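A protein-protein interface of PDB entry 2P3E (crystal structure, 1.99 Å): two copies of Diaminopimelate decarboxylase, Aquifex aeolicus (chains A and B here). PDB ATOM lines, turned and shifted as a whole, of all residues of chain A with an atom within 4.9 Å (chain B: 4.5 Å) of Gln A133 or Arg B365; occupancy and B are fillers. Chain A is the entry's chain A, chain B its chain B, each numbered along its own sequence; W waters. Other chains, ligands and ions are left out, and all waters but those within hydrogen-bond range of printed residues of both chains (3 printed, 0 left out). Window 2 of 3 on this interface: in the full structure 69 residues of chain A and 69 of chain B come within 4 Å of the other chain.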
ATOM      1  N   GLU A 113      -7.047  -2.919  -3.116  1.00  0.00           N
ATOM      2  CA  GLU A 113      -6.525  -3.260  -4.443  1.00  0.00           C
ATOM      3  C   GLU A 113      -6.050  -2.001  -5.192  1.00  0.00           C
ATOM      4  O   GLU A 113      -4.956  -1.989  -5.752  1.00  0.00           O
ATOM      5  CB  GLU A 113      -7.588  -4.013  -5.261  1.00  0.00           C
ATOM      6  CG  GLU A 113      -7.102  -4.555  -6.596  1.00  0.00           C
ATOM      7  CD  GLU A 113      -6.359  -5.870  -6.485  1.00  0.00           C
ATOM      8  OE1 GLU A 113      -6.217  -6.416  -5.356  1.00  0.00           O
ATOM      9  OE2 GLU A 113      -5.917  -6.374  -7.550  1.00  0.00           O
ATOM     10  N   SER A 131       1.040  -9.311   6.102  1.00  0.00           N
ATOM     11  CA  SER A 131       0.377 -10.624   6.029  1.00  0.00           C
ATOM     12  C   SER A 131       0.879 -11.427   4.838  1.00  0.00           C
ATOM     13  O   SER A 131       1.358 -10.866   3.856  1.00  0.00           O
ATOM     14  CB  SER A 131      -1.154 -10.496   5.973  1.00  0.00           C
ATOM     15  OG  SER A 131      -1.611  -9.895   4.762  1.00  0.00           O
ATOM     16  N   ARG A 132       0.781 -12.750   4.936  1.00  0.00           N
ATOM     17  CA  ARG A 132       1.035 -13.599   3.781  1.00  0.00           C
ATOM     18  C   ARG A 132       0.075 -13.305   2.610  1.00  0.00           C
ATOM     19  O   ARG A 132       0.502 -13.245   1.447  1.00  0.00           O
ATOM     20  CB  ARG A 132       0.953 -15.064   4.179  1.00  0.00           C
ATOM     21  CG  ARG A 132       1.271 -15.989   3.003  1.00  0.00           C
ATOM     22  CD  ARG A 132       1.563 -17.392   3.470  1.00  0.00           C
ATOM     23  NE  ARG A 132       2.684 -17.445   4.411  1.00  0.00           N
ATOM     24  CZ  ARG A 132       3.303 -18.575   4.749  1.00  0.00           C
ATOM     25  NH1 ARG A 132       2.908 -19.720   4.213  1.00  0.00           N
ATOM     26  NH2 ARG A 132       4.310 -18.561   5.614  1.00  0.00           N
ATOM     27  N   GLN A 133      -1.214 -13.116   2.905  1.00  0.00           N
ATOM     28  CA  GLN A 133      -2.167 -12.790   1.861  1.00  0.00           C
ATOM     29  C   GLN A 133      -1.750 -11.536   1.089  1.00  0.00           C
ATOM     30  O   GLN A 133      -1.914 -11.472  -0.134  1.00  0.00           O
ATOM     31  CB  GLN A 133      -3.576 -12.631   2.421  1.00  0.00           C
ATOM     32  CG  GLN A 133      -4.650 -12.654   1.344  1.00  0.00           C
ATOM     33  CD  GLN A 133      -6.011 -13.045   1.890  1.00  0.00           C
ATOM     34  OE1 GLN A 133      -6.357 -12.698   3.011  1.00  0.00           O
ATOM     35  NE2 GLN A 133      -6.788 -13.774   1.088  1.00  0.00           N
ATOM     36  N   GLU A 134      -1.207 -10.557   1.814  1.00  0.00           N
ATOM     37  CA  GLU A 134      -0.700  -9.331   1.202  1.00  0.00           C
ATOM     38  C   GLU A 134       0.436  -9.659   0.222  1.00  0.00           C
ATOM     39  O   GLU A 134       0.510  -9.069  -0.850  1.00  0.00           O
ATOM     40  CB  GLU A 134      -0.214  -8.326   2.263  1.00  0.00           C
ATOM     41  CG  GLU A 134       0.275  -6.983   1.651  1.00  0.00           C
ATOM     42  CD  GLU A 134       0.918  -6.042   2.668  1.00  0.00           C
ATOM     43  OE1 GLU A 134       0.615  -6.148   3.881  1.00  0.00           O
ATOM     44  OE2 GLU A 134       1.730  -5.182   2.239  1.00  0.00           O
ATOM     45  N   LEU A 135       1.304 -10.607   0.583  1.00  0.00           N
ATOM     46  CA  LEU A 135       2.334 -11.071  -0.360  1.00  0.00           C
ATOM     47  C   LEU A 135       1.708 -11.581  -1.668  1.00  0.00           C
ATOM     48  O   LEU A 135       2.146 -11.200  -2.758  1.00  0.00           O
ATOM     49  CB  LEU A 135       3.240 -12.156   0.271  1.00  0.00           C
ATOM     50  CG  LEU A 135       4.166 -11.784   1.432  1.00  0.00           C
ATOM     51  CD1 LEU A 135       4.721 -13.049   2.119  1.00  0.00           C
ATOM     52  CD2 LEU A 135       5.308 -10.891   0.943  1.00  0.00           C
ATOM     53  N   ASP A 136       0.691 -12.445  -1.551  1.00  0.00           N
ATOM     54  CA  ASP A 136      -0.030 -12.982  -2.715  1.00  0.00           C
ATOM     55  C   ASP A 136      -0.701 -11.878  -3.549  1.00  0.00           C
ATOM     56  O   ASP A 136      -0.624 -11.885  -4.783  1.00  0.00           O
ATOM     57  CB  ASP A 136      -1.081 -14.018  -2.278  1.00  0.00           C
ATOM     58  CG  ASP A 136      -0.459 -15.266  -1.665  1.00  0.00           C
ATOM     59  OD1 ASP A 136       0.633 -15.678  -2.119  1.00  0.00           O
ATOM     60  OD2 ASP A 136      -1.050 -15.829  -0.717  1.00  0.00           O
ATOM     61  N   VAL A 137      -1.350 -10.930  -2.867  1.00  0.00           N
ATOM     62  CA  VAL A 137      -2.034  -9.810  -3.536  1.00  0.00           C
ATOM     63  C   VAL A 137      -1.035  -8.923  -4.292  1.00  0.00           C
ATOM     64  O   VAL A 137      -1.242  -8.600  -5.475  1.00  0.00           O
ATOM     65  CB  VAL A 137      -2.870  -8.947  -2.516  1.00  0.00           C
ATOM     66  CG1 VAL A 137      -3.445  -7.707  -3.201  1.00  0.00           C
ATOM     67  CG2 VAL A 137      -4.005  -9.777  -1.934  1.00  0.00           C
ATOM     68  N   VAL B 295     -13.982  -7.121   3.236  1.00  0.00           N
ATOM     69  CA  VAL B 295     -12.827  -7.841   3.753  1.00  0.00           C
ATOM     70  C   VAL B 295     -11.654  -7.732   2.764  1.00  0.00           C
ATOM     71  O   VAL B 295     -11.802  -8.027   1.572  1.00  0.00           O
ATOM     72  CB  VAL B 295     -13.160  -9.343   4.037  1.00  0.00           C
ATOM     73  CG1 VAL B 295     -11.897 -10.081   4.522  1.00  0.00           C
ATOM     74  CG2 VAL B 295     -14.309  -9.478   5.057  1.00  0.00           C
ATOM     75  N   GLN B 296     -10.508  -7.275   3.269  1.00  0.00           N
ATOM     76  CA  GLN B 296      -9.300  -7.081   2.479  1.00  0.00           C
ATOM     77  C   GLN B 296      -8.332  -8.233   2.704  1.00  0.00           C
ATOM     78  O   GLN B 296      -7.845  -8.815   1.736  1.00  0.00           O
ATOM     79  CB  GLN B 296      -8.631  -5.749   2.831  1.00  0.00           C
ATOM     80  CG  GLN B 296      -9.517  -4.528   2.625  1.00  0.00           C
ATOM     81  CD  GLN B 296     -10.108  -4.448   1.228  1.00  0.00           C
ATOM     82  OE1 GLN B 296      -9.381  -4.442   0.230  1.00  0.00           O
ATOM     83  NE2 GLN B 296     -11.435  -4.392   1.146  1.00  0.00           N
ATOM     84  N   PHE B 297      -8.074  -8.575   3.971  1.00  0.00           N
ATOM     85  CA  PHE B 297      -7.131  -9.651   4.305  1.00  0.00           C
ATOM     86  C   PHE B 297      -7.617 -10.482   5.490  1.00  0.00           C
ATOM     87  O   PHE B 297      -8.311  -9.968   6.377  1.00  0.00           O
ATOM     88  CB  PHE B 297      -5.739  -9.100   4.656  1.00  0.00           C
ATOM     89  CG  PHE B 297      -5.149  -8.210   3.606  1.00  0.00           C
ATOM     90  CD1 PHE B 297      -4.577  -8.743   2.460  1.00  0.00           C
ATOM     91  CD2 PHE B 297      -5.173  -6.832   3.766  1.00  0.00           C
ATOM     92  CE1 PHE B 297      -4.035  -7.896   1.471  1.00  0.00           C
ATOM     93  CE2 PHE B 297      -4.630  -5.989   2.793  1.00  0.00           C
ATOM     94  CZ  PHE B 297      -4.056  -6.530   1.646  1.00  0.00           C
ATOM     95  N   LEU B 298      -7.242 -11.764   5.487  1.00  0.00           N
ATOM     96  CA  LEU B 298      -7.278 -12.609   6.689  1.00  0.00           C
ATOM     97  C   LEU B 298      -5.847 -12.852   7.128  1.00  0.00           C
ATOM     98  O   LEU B 298      -4.960 -13.045   6.292  1.00  0.00           O
ATOM     99  CB  LEU B 298      -7.961 -13.957   6.420  1.00  0.00           C
ATOM    100  CG  LEU B 298      -9.367 -13.938   5.808  1.00  0.00           C
ATOM    101  CD1 LEU B 298      -9.814 -15.366   5.485  1.00  0.00           C
ATOM    102  CD2 LEU B 298     -10.399 -13.252   6.723  1.00  0.00           C
ATOM    103  N   GLN B 364     -14.321 -14.493   3.493  1.00  0.00           N
ATOM    104  CA  GLN B 364     -13.088 -14.428   2.714  1.00  0.00           C
ATOM    105  C   GLN B 364     -12.846 -13.033   2.137  1.00  0.00           C
ATOM    106  O   GLN B 364     -13.754 -12.195   2.125  1.00  0.00           O
ATOM    107  CB  GLN B 364     -13.105 -15.486   1.601  1.00  0.00           C
ATOM    108  CG  GLN B 364     -13.135 -16.965   2.129  1.00  0.00           C
ATOM    109  CD  GLN B 364     -11.958 -17.316   3.048  1.00  0.00           C
ATOM    110  OE1 GLN B 364     -10.800 -17.331   2.621  1.00  0.00           O
ATOM    111  NE2 GLN B 364     -12.256 -17.600   4.324  1.00  0.00           N
ATOM    112  N   ARG B 365     -11.623 -12.814   1.651  1.00  0.00           N
ATOM    113  CA  ARG B 365     -11.260 -11.585   0.969  1.00  0.00           C
ATOM    114  C   ARG B 365     -12.281 -11.294  -0.141  1.00  0.00           C
ATOM    115  O   ARG B 365     -12.627 -12.188  -0.915  1.00  0.00           O
ATOM    116  CB  ARG B 365      -9.835 -11.701   0.394  1.00  0.00           C
ATOM    117  CG  ARG B 365      -9.431 -10.542  -0.520  1.00  0.00           C
ATOM    118  CD  ARG B 365      -7.897 -10.421  -0.690  1.00  0.00           C
ATOM    119  NE  ARG B 365      -7.492  -9.041  -1.041  1.00  0.00           N
ATOM    120  CZ  ARG B 365      -7.372  -8.628  -2.294  1.00  0.00           C
ATOM    121  NH1 ARG B 365      -7.630  -9.484  -3.264  1.00  0.00           N
ATOM    122  NH2 ARG B 365      -6.998  -7.392  -2.586  1.00  0.00           N
ATOM    123  N   GLY B 366     -12.785 -10.059  -0.181  1.00  0.00           N
ATOM    124  CA  GLY B 366     -13.739  -9.633  -1.207  1.00  0.00           C
ATOM    125  C   GLY B 366     -15.191  -9.656  -0.729  1.00  0.00           C
ATOM    126  O   GLY B 366     -16.052  -8.969  -1.292  1.00  0.00           O
ATOM    127  N   GLU B 367     -15.472 -10.446   0.307  1.00  0.00           N
ATOM    128  CA  GLU B 367     -16.826 -10.508   0.867  1.00  0.00           C
ATOM    129  C   GLU B 367     -17.133  -9.245   1.663  1.00  0.00           C
ATOM    130  O   GLU B 367     -16.220  -8.599   2.161  1.00  0.00           O
ATOM    131  CB  GLU B 367     -16.971 -11.692   1.810  1.00  0.00           C
ATOM    132  CG  GLU B 367     -17.209 -13.010   1.133  1.00  0.00           C
ATOM    133  CD  GLU B 367     -17.577 -14.071   2.141  1.00  0.00           C
ATOM    134  OE1 GLU B 367     -18.693 -14.022   2.723  1.00  0.00           O
ATOM    135  OE2 GLU B 367     -16.736 -14.947   2.355  1.00  0.00           O
HETATM  136  O   HOH W   1      -9.603  -4.163  -2.282  1.00  0.00           O
HETATM  137  O   HOH W   2      -9.596 -14.956   1.832  1.00  0.00           O
HETATM  138  O   HOH W   3      -2.461 -13.966   5.571  1.00  0.00           O
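OE1 of Glu A113 lies within salt-bridge range of NH2 of Arg B365 (3.0 Å). OE1 of Gln A133 is in hydrogen-bond range of N of Leu B298 (2.8 Å).
The side-chain hydroxyl of Ser A131 sits at hydrogen-bond distance from the backbone NH of Glu A134. O of Gln B296 lies within hydrogen-bond range of NE of Arg B365 (2.8 Å).
Among the printed residues, merely in contact across the chains: Gln A133 with Phe B297 (3.4 Å), Val A137 with Arg B365 (3.6 Å), Glu A134 with Phe B297 (3.6 Å), Gln A133 with Arg B365 (3.8 Å), Val A137 with Phe B297 (3.9 Å) and Ser A131 with Phe B297 (3.9 Å).
Of the printed residues of chain B, Glu A113 touches Arg B365 (3.0 Å). Of the printed residues of chain B, Ser A131 touches Phe B297 (3.9 Å). Of chain B, only Phe B297, Leu B298 and Arg B365 come within 4 Å of Gln A133. Leu A135 touches none of the printed residues of chain B. Of the printed residues of chain B, Val A137 touches Phe B297 and Arg B365. Of the printed residues of chain A, Phe B297 touches Ser A131, Gln A133, Glu A134 and Val A137. Printed residues of chain A within 4 Å of Leu B298: Gln A133 (2.8 Å). Of chain A, only Glu A113 (3.0 Å), Gln A133 (3.8 Å) and Val A137 (3.6 Å) come within 4 Å of Arg B365. Glu B367 touches none of the printed residues of chain A. The nearest printed residue of chain A that does not touch Arg B365 is Glu A134 (7.1 Å).
Along chain A the printed residues that touch a printed residue of chain B span positions 113 to 137. Of the 8 printed residues of chain B, 3 touch a printed residue of chain A. Hydrophobic or aromatic side chains of chain B within 4 Å of the printed part of chain A: Phe B297 and Leu B298. Among the printed residues, 8 pairs touch across the chains. Among the printed residues, Asp or Glu carboxylates within 4 Å of a Lys or Arg side-chain nitrogen of the other chain: Glu A113 with Arg B365 (3.0 Å).
No position is printed for both chains.
Water W1 bridges OE1 of Gln B296 (2.5 Å) and N of Glu A113 (3.0 Å). Water W3 lies within hydrogen-bond range of the backbone carbonyl oxygen of Leu B298 and the backbone NH of Gln A133. Water W2 lies within hydrogen-bond range of the side-chain amide oxygen of Gln B364, the backbone NH of Arg B365 and the side-chain amide nitrogen of Gln A133.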
